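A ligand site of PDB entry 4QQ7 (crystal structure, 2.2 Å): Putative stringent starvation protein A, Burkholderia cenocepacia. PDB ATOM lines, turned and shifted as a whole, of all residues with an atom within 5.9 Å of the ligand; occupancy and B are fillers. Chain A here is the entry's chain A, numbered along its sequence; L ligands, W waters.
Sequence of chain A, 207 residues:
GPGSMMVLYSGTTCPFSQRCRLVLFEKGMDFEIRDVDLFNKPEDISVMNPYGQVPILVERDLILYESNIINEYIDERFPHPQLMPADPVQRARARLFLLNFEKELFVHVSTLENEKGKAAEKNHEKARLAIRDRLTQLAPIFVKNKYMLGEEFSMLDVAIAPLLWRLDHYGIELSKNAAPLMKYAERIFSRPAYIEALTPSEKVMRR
Water W4 bridges an oxygen (O5) of the ligand (2.7 Å) and the side-chain amide nitrogen (NE2) of Gln 53 (3.3 Å). Water W2 lies within hydrogen-bond range of the side-chain hydroxyl (OG) of Ser 110 (2.7 Å), an oxygen (O3) of the ligand (2.8 Å), the side-chain amide nitrogen (NE2) of Gln 53 (3.3 Å) and the side-chain amide nitrogen (ND2) of Asn 114 (3.4 Å). Water W1 lies within hydrogen-bond range of an oxygen (O2) of the ligand (2.8 Å), the backbone carbonyl oxygen of Pro 55 (2.8 Å) and the backbone NH of Glu 66 (2.8 Å). Water W3 lies within hydrogen-bond range of O1 of the ligand (3.0 Å), N of Asn 68 (3.1 Å), OG of Ser 67 (3.2 Å) and OE1 of Glu 102 (3.5 Å).
An oxygen (O2) of the ligand sits at hydrogen-bond distance from the backbone NH (N) of Ser 67 (2.8 Å). The side-chain hydroxyl of Ser 67 lies within hydrogen-bond range of an oxygen (O1) of the ligand, 2.5 Å away. The backbone NH (N) of Val 54 lies within hydrogen-bond range of an oxygen (O4) of the ligand. The backbone carbonyl oxygen (O) of Val 54 is in hydrogen-bond range of a nitrogen (N2) of the ligand, 2.8 Å away. The side-chain amino group (NZ) of Lys 41 is in salt-bridge range of an oxygen (O6) of the ligand (2.8 Å). The side-chain carboxylate (OE1) of Glu 66 is in salt-bridge range of a nitrogen (N1) of the ligand (2.8 Å). The side-chain amide nitrogen (NE2) of Gln 53 lies within hydrogen-bond range of an oxygen (O3) of the ligand (3.3 Å). The side-chain amide oxygen (OD1) of Asn 114 lies within hydrogen-bond range of a nitrogen (N3) of the ligand (3.2 Å). The side-chain sulfur (SG) of Cys 14 sits close to a sulfur (S1) of the ligand (3.4 Å).
Residues that only touch the ligand: Pro 15 (3.9 Å), Phe 16 (3.1 Å), Leu 38 (3.6 Å), Gly 52 (3.4 Å), Pro 55 (3.4 Å) and Glu 113 (3.8 Å). Of the 21 residues printed, 13 come within 4 Å of the ligand.
The guanidinium group (NH1) of Arg 19 sits at hydrogen-bond distance from the side-chain hydroxyl (OG) of Ser 67. NZ of Lys 41 lies within hydrogen-bond range of O of Gly 52 (2.9 Å). The side-chain sulfur (SG) of Cys 14 sits close to the backbone NH (N) of Phe 16. ND2 of Asn 114 lies close to O of Ser 110, at 3.3 Å. O of Glu 113 sits at hydrogen-bond distance from NZ of Lys 116.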
ATOM      1  N   THR A  13       5.243 -27.612 -19.938  1.00  0.00           N
ATOM      2  CA  THR A  13       4.914 -28.896 -20.543  1.00  0.00           C
ATOM      3  C   THR A  13       4.416 -28.698 -21.968  1.00  0.00           C
ATOM      4  O   THR A  13       3.767 -29.575 -22.527  1.00  0.00           O
ATOM      5  CB  THR A  13       3.859 -29.660 -19.756  1.00  0.00           C
ATOM      6  OG1 THR A  13       2.673 -28.855 -19.664  1.00  0.00           O
ATOM      7  CG2 THR A  13       4.365 -29.981 -18.342  1.00  0.00           C
ATOM      8  N   CYS A  14       4.706 -27.532 -22.535  1.00  0.00           N
ATOM      9  CA  CYS A  14       4.267 -27.218 -23.889  1.00  0.00           C
ATOM     10  C   CYS A  14       5.133 -27.897 -24.924  1.00  0.00           C
ATOM     11  O   CYS A  14       6.327 -27.629 -24.979  1.00  0.00           O
ATOM     12  CB  CYS A  14       4.285 -25.708 -24.127  1.00  0.00           C
ATOM     13  SG  CYS A  14       4.045 -25.263 -25.884  1.00  0.00           S
ATOM     14  N   PRO A  15       4.555 -28.776 -25.754  1.00  0.00           N
ATOM     15  CA  PRO A  15       5.412 -29.511 -26.700  1.00  0.00           C
ATOM     16  C   PRO A  15       6.007 -28.573 -27.746  1.00  0.00           C
ATOM     17  O   PRO A  15       7.081 -28.821 -28.279  1.00  0.00           O
ATOM     18  CB  PRO A  15       4.471 -30.529 -27.342  1.00  0.00           C
ATOM     19  CG  PRO A  15       3.029 -29.964 -27.078  1.00  0.00           C
ATOM     20  CD  PRO A  15       3.144 -29.217 -25.777  1.00  0.00           C
ATOM     21  N   PHE A  16       5.283 -27.518 -28.071  1.00  0.00           N
ATOM     22  CA  PHE A  16       5.820 -26.562 -29.023  1.00  0.00           C
ATOM     23  C   PHE A  16       7.018 -25.803 -28.452  1.00  0.00           C
ATOM     24  O   PHE A  16       8.045 -25.579 -29.131  1.00  0.00           O
ATOM     25  CB  PHE A  16       4.720 -25.602 -29.451  1.00  0.00           C
ATOM     26  CG  PHE A  16       3.586 -26.285 -30.163  1.00  0.00           C
ATOM     27  CD1 PHE A  16       3.698 -26.617 -31.512  1.00  0.00           C
ATOM     28  CD2 PHE A  16       2.413 -26.629 -29.481  1.00  0.00           C
ATOM     29  CE1 PHE A  16       2.657 -27.247 -32.180  1.00  0.00           C
ATOM     30  CE2 PHE A  16       1.370 -27.266 -30.143  1.00  0.00           C
ATOM     31  CZ  PHE A  16       1.504 -27.571 -31.514  1.00  0.00           C
ATOM     32  N   ARG A  19      10.306 -27.814 -28.578  1.00  0.00           N
ATOM     33  CA  ARG A  19      11.039 -27.724 -29.837  1.00  0.00           C
ATOM     34  C   ARG A  19      12.107 -26.635 -29.721  1.00  0.00           C
ATOM     35  O   ARG A  19      13.293 -26.862 -30.025  1.00  0.00           O
ATOM     36  CB  ARG A  19      10.106 -27.395 -31.010  1.00  0.00           C
ATOM     37  CG  ARG A  19       9.046 -28.410 -31.317  1.00  0.00           C
ATOM     38  CD  ARG A  19       8.132 -27.854 -32.399  1.00  0.00           C
ATOM     39  NE  ARG A  19       7.357 -28.894 -33.057  1.00  0.00           N
ATOM     40  CZ  ARG A  19       6.391 -28.636 -33.937  1.00  0.00           C
ATOM     41  NH1 ARG A  19       6.051 -27.386 -34.212  1.00  0.00           N
ATOM     42  NH2 ARG A  19       5.742 -29.656 -34.518  1.00  0.00           N
ATOM     43  N   LEU A  38       0.884 -21.924 -17.791  1.00  0.00           N
ATOM     44  CA  LEU A  38      -0.297 -21.786 -18.643  1.00  0.00           C
ATOM     45  C   LEU A  38      -1.620 -22.015 -17.895  1.00  0.00           C
ATOM     46  O   LEU A  38      -2.687 -21.857 -18.488  1.00  0.00           O
ATOM     47  CB  LEU A  38      -0.197 -22.761 -19.808  1.00  0.00           C
ATOM     48  CG  LEU A  38       0.829 -22.368 -20.882  1.00  0.00           C
ATOM     49  CD1 LEU A  38       0.847 -23.376 -22.050  1.00  0.00           C
ATOM     50  CD2 LEU A  38       0.512 -20.967 -21.379  1.00  0.00           C
ATOM     51  N   LYS A  41      -1.832 -17.941 -16.981  1.00  0.00           N
ATOM     52  CA  LYS A  41      -1.083 -17.255 -18.045  1.00  0.00           C
ATOM     53  C   LYS A  41      -1.016 -15.745 -17.838  1.00  0.00           C
ATOM     54  O   LYS A  41      -2.057 -15.078 -17.716  1.00  0.00           O
ATOM     55  CB  LYS A  41      -1.716 -17.586 -19.399  1.00  0.00           C
ATOM     56  CG  LYS A  41      -0.991 -16.998 -20.596  1.00  0.00           C
ATOM     57  CD  LYS A  41      -1.499 -17.594 -21.900  1.00  0.00           C
ATOM     58  CE  LYS A  41      -2.974 -17.317 -22.123  1.00  0.00           C
ATOM     59  NZ  LYS A  41      -3.488 -18.015 -23.344  1.00  0.00           N
ATOM     60  N   TYR A  51      -2.142 -14.273 -30.432  1.00  0.00           N
ATOM     61  CA  TYR A  51      -2.819 -15.563 -30.327  1.00  0.00           C
ATOM     62  C   TYR A  51      -2.742 -16.115 -28.895  1.00  0.00           C
ATOM     63  O   TYR A  51      -3.340 -17.162 -28.585  1.00  0.00           O
ATOM     64  CB  TYR A  51      -2.232 -16.563 -31.319  1.00  0.00           C
ATOM     65  CG  TYR A  51      -2.437 -16.135 -32.761  1.00  0.00           C
ATOM     66  CD1 TYR A  51      -3.657 -16.342 -33.397  1.00  0.00           C
ATOM     67  CD2 TYR A  51      -1.421 -15.511 -33.472  1.00  0.00           C
ATOM     68  CE1 TYR A  51      -3.860 -15.942 -34.717  1.00  0.00           C
ATOM     69  CE2 TYR A  51      -1.614 -15.100 -34.792  1.00  0.00           C
ATOM     70  CZ  TYR A  51      -2.834 -15.324 -35.402  1.00  0.00           C
ATOM     71  OH  TYR A  51      -3.017 -14.913 -36.702  1.00  0.00           O
ATOM     72  N   GLY A  52      -2.038 -15.387 -28.025  1.00  0.00           N
ATOM     73  CA  GLY A  52      -1.907 -15.722 -26.625  1.00  0.00           C
ATOM     74  C   GLY A  52      -1.205 -17.036 -26.352  1.00  0.00           C
ATOM     75  O   GLY A  52      -1.447 -17.685 -25.344  1.00  0.00           O
ATOM     76  N   GLN A  53      -0.280 -17.422 -27.239  1.00  0.00           N
ATOM     77  CA  GLN A  53       0.375 -18.700 -27.079  1.00  0.00           C
ATOM     78  C   GLN A  53       1.867 -18.572 -26.842  1.00  0.00           C
ATOM     79  O   GLN A  53       2.517 -17.583 -27.201  1.00  0.00           O
ATOM     80  CB  GLN A  53       0.147 -19.610 -28.307  1.00  0.00           C
ATOM     81  CG  GLN A  53      -1.296 -20.071 -28.486  1.00  0.00           C
ATOM     82  CD  GLN A  53      -1.524 -20.713 -29.844  1.00  0.00           C
ATOM     83  OE1 GLN A  53      -0.791 -20.451 -30.789  1.00  0.00           O
ATOM     84  NE2 GLN A  53      -2.547 -21.568 -29.930  1.00  0.00           N
ATOM     85  N   VAL A  54       2.372 -19.617 -26.224  1.00  0.00           N
ATOM     86  CA  VAL A  54       3.783 -19.827 -26.039  1.00  0.00           C
ATOM     87  C   VAL A  54       4.108 -20.955 -27.028  1.00  0.00           C
ATOM     88  O   VAL A  54       3.197 -21.728 -27.354  1.00  0.00           O
ATOM     89  CB  VAL A  54       3.999 -20.165 -24.553  1.00  0.00           C
ATOM     90  CG1 VAL A  54       3.827 -21.619 -24.271  1.00  0.00           C
ATOM     91  CG2 VAL A  54       5.245 -19.577 -24.004  1.00  0.00           C
ATOM     92  N   PRO A  55       5.361 -21.056 -27.538  1.00  0.00           N
ATOM     93  CA  PRO A  55       6.561 -20.246 -27.262  1.00  0.00           C
ATOM     94  C   PRO A  55       6.557 -18.872 -27.905  1.00  0.00           C
ATOM     95  O   PRO A  55       5.918 -18.653 -28.937  1.00  0.00           O
ATOM     96  CB  PRO A  55       7.694 -21.111 -27.821  1.00  0.00           C
ATOM     97  CG  PRO A  55       7.044 -21.901 -28.958  1.00  0.00           C
ATOM     98  CD  PRO A  55       5.659 -22.180 -28.455  1.00  0.00           C
ATOM     99  N   TYR A  65       6.732 -15.531 -32.579  1.00  0.00           N
ATOM    100  CA  TYR A  65       6.051 -16.700 -32.048  1.00  0.00           C
ATOM    101  C   TYR A  65       5.901 -17.687 -33.199  1.00  0.00           C
ATOM    102  O   TYR A  65       6.334 -17.356 -34.316  1.00  0.00           O
ATOM    103  CB  TYR A  65       4.711 -16.327 -31.399  1.00  0.00           C
ATOM    104  CG  TYR A  65       3.892 -15.370 -32.217  1.00  0.00           C
ATOM    105  CD1 TYR A  65       3.013 -15.859 -33.166  1.00  0.00           C
ATOM    106  CD2 TYR A  65       4.001 -13.991 -32.051  1.00  0.00           C
ATOM    107  CE1 TYR A  65       2.258 -15.014 -33.935  1.00  0.00           C
ATOM    108  CE2 TYR A  65       3.244 -13.118 -32.835  1.00  0.00           C
ATOM    109  CZ  TYR A  65       2.367 -13.634 -33.768  1.00  0.00           C
ATOM    110  OH  TYR A  65       1.605 -12.819 -34.558  1.00  0.00           O
ATOM    111  N   GLU A  66       5.259 -18.833 -32.907  1.00  0.00           N
ATOM    112  CA  GLU A  66       5.214 -20.024 -33.778  1.00  0.00           C
ATOM    113  C   GLU A  66       6.555 -20.752 -33.718  1.00  0.00           C
ATOM    114  O   GLU A  66       7.552 -20.263 -34.249  1.00  0.00           O
ATOM    115  CB  GLU A  66       4.856 -19.666 -35.225  1.00  0.00           C
ATOM    116  CG  GLU A  66       3.536 -18.946 -35.362  1.00  0.00           C
ATOM    117  CD  GLU A  66       2.363 -19.818 -34.994  1.00  0.00           C
ATOM    118  OE1 GLU A  66       2.407 -21.021 -35.329  1.00  0.00           O
ATOM    119  OE2 GLU A  66       1.416 -19.310 -34.345  1.00  0.00           O
ATOM    120  N   SER A  67       6.571 -21.903 -33.068  1.00  0.00           N
ATOM    121  CA  SER A  67       7.821 -22.622 -32.782  1.00  0.00           C
ATOM    122  C   SER A  67       8.738 -22.815 -34.009  1.00  0.00           C
ATOM    123  O   SER A  67       9.946 -22.575 -33.923  1.00  0.00           O
ATOM    124  CB  SER A  67       7.507 -23.983 -32.135  1.00  0.00           C
ATOM    125  OG  SER A  67       6.553 -24.680 -32.928  1.00  0.00           O
ATOM    126  N   ASN A  68       8.186 -23.225 -35.150  1.00  0.00           N
ATOM    127  CA  ASN A  68       9.000 -23.437 -36.339  1.00  0.00           C
ATOM    128  C   ASN A  68       9.596 -22.149 -36.917  1.00  0.00           C
ATOM    129  O   ASN A  68      10.706 -22.167 -37.457  1.00  0.00           O
ATOM    130  CB  ASN A  68       8.191 -24.193 -37.412  1.00  0.00           C
ATOM    131  CG  ASN A  68       8.046 -25.694 -37.067  1.00  0.00           C
ATOM    132  OD1 ASN A  68       8.670 -26.161 -36.116  1.00  0.00           O
ATOM    133  ND2 ASN A  68       7.226 -26.423 -37.821  1.00  0.00           N
ATOM    134  N   GLU A 102       2.838 -30.299 -39.384  1.00  0.00           N
ATOM    135  CA  GLU A 102       1.935 -29.414 -38.683  1.00  0.00           C
ATOM    136  C   GLU A 102       0.503 -29.768 -39.046  1.00  0.00           C
ATOM    137  O   GLU A 102      -0.360 -29.842 -38.176  1.00  0.00           O
ATOM    138  CB  GLU A 102       2.216 -27.937 -38.997  1.00  0.00           C
ATOM    139  CG  GLU A 102       3.574 -27.454 -38.498  1.00  0.00           C
ATOM    140  CD  GLU A 102       3.779 -27.649 -37.010  1.00  0.00           C
ATOM    141  OE1 GLU A 102       3.177 -26.897 -36.224  1.00  0.00           O
ATOM    142  OE2 GLU A 102       4.488 -28.594 -36.614  1.00  0.00           O
ATOM    143  N   SER A 110      -2.415 -29.836 -30.958  1.00  0.00           N
ATOM    144  CA  SER A 110      -3.052 -28.595 -30.525  1.00  0.00           C
ATOM    145  C   SER A 110      -4.405 -28.881 -29.927  1.00  0.00           C
ATOM    146  O   SER A 110      -4.805 -28.257 -28.943  1.00  0.00           O
ATOM    147  CB  SER A 110      -3.224 -27.603 -31.694  1.00  0.00           C
ATOM    148  OG  SER A 110      -1.990 -27.037 -32.048  1.00  0.00           O
ATOM    149  N   GLU A 113      -3.796 -30.325 -26.578  1.00  0.00           N
ATOM    150  CA  GLU A 113      -3.229 -29.428 -25.593  1.00  0.00           C
ATOM    151  C   GLU A 113      -4.176 -28.296 -25.197  1.00  0.00           C
ATOM    152  O   GLU A 113      -4.249 -27.914 -24.027  1.00  0.00           O
ATOM    153  CB  GLU A 113      -1.912 -28.828 -26.096  1.00  0.00           C
ATOM    154  CG  GLU A 113      -0.781 -29.831 -26.183  1.00  0.00           C
ATOM    155  CD  GLU A 113      -0.260 -30.235 -24.827  1.00  0.00           C
ATOM    156  OE1 GLU A 113      -0.523 -29.502 -23.846  1.00  0.00           O
ATOM    157  OE2 GLU A 113       0.402 -31.288 -24.719  1.00  0.00           O
ATOM    158  N   ASN A 114      -4.903 -27.768 -26.173  1.00  0.00           N
ATOM    159  CA  ASN A 114      -5.604 -26.497 -26.004  1.00  0.00           C
ATOM    160  C   ASN A 114      -7.100 -26.639 -25.720  1.00  0.00           C
ATOM    161  O   ASN A 114      -7.673 -25.820 -25.003  1.00  0.00           O
ATOM    162  CB  ASN A 114      -5.366 -25.633 -27.247  1.00  0.00           C
ATOM    163  CG  ASN A 114      -3.890 -25.253 -27.423  1.00  0.00           C
ATOM    164  OD1 ASN A 114      -3.157 -25.027 -26.446  1.00  0.00           O
ATOM    165  ND2 ASN A 114      -3.434 -25.225 -28.673  1.00  0.00           N
ATOM    166  N   LYS A 116     -10.194 -28.123 -23.843  1.00  0.00           N
ATOM    167  CA  LYS A 116     -10.390 -28.689 -22.514  1.00  0.00           C
ATOM    168  C   LYS A 116     -11.864 -28.963 -22.233  1.00  0.00           C
ATOM    169  O   LYS A 116     -12.732 -28.603 -23.027  1.00  0.00           O
ATOM    170  CB  LYS A 116      -9.825 -27.745 -21.447  1.00  0.00           C
ATOM    171  CG  LYS A 116      -8.385 -28.030 -21.075  1.00  0.00           C
ATOM    172  CD  LYS A 116      -7.419 -27.063 -21.756  1.00  0.00           C
ATOM    173  CE  LYS A 116      -5.989 -27.412 -21.413  1.00  0.00           C
ATOM    174  NZ  LYS A 116      -5.054 -26.322 -21.798  1.00  0.00           N
HETATM  175  N1  LIG L   1       1.623 -23.293 -33.825  1.00  0.00           N
HETATM  176  C1  LIG L   1       2.085 -22.857 -32.531  1.00  0.00           C
HETATM  177  C2  LIG L   1       3.547 -23.125 -32.394  1.00  0.00           C
HETATM  178  O1  LIG L   1       4.119 -23.987 -33.129  1.00  0.00           O
HETATM  179  O2  LIG L   1       4.243 -22.452 -31.588  1.00  0.00           O
HETATM  180  C3  LIG L   1       1.216 -23.514 -31.426  1.00  0.00           C
HETATM  181  C4  LIG L   1       1.678 -23.060 -30.004  1.00  0.00           C
HETATM  182  C5  LIG L   1       0.634 -23.484 -28.971  1.00  0.00           C
HETATM  183  O3  LIG L   1      -0.427 -23.963 -29.308  1.00  0.00           O
HETATM  184  N2  LIG L   1       0.932 -23.323 -27.561  1.00  0.00           N
HETATM  185  C6  LIG L   1      -0.039 -23.687 -26.530  1.00  0.00           C
HETATM  186  C7  LIG L   1      -0.513 -22.410 -25.851  1.00  0.00           C
HETATM  187  O4  LIG L   1       0.288 -21.526 -25.604  1.00  0.00           O
HETATM  188  C8  LIG L   1       0.588 -24.521 -25.483  1.00  0.00           C
HETATM  189  S1  LIG L   1       0.774 -26.175 -26.107  1.00  0.00           S
HETATM  190  N3  LIG L   1      -1.905 -22.230 -25.480  1.00  0.00           N
HETATM  191  C9  LIG L   1      -2.238 -20.963 -24.830  1.00  0.00           C
HETATM  192  C10 LIG L   1      -3.510 -21.070 -24.006  1.00  0.00           C
HETATM  193  O5  LIG L   1      -4.587 -21.448 -24.542  1.00  0.00           O
HETATM  194  O6  LIG L   1      -3.474 -20.753 -22.797  1.00  0.00           O
HETATM  195  O   HOH W   1       4.020 -19.850 -30.606  1.00  0.00           O
HETATM  196  O   HOH W   2      -1.953 -24.360 -31.605  1.00  0.00           O
HETATM  197  O   HOH W   3       5.306 -24.198 -35.885  1.00  0.00           O
HETATM  198  O   HOH W   4      -4.492 -21.721 -27.271  1.00  0.00           O
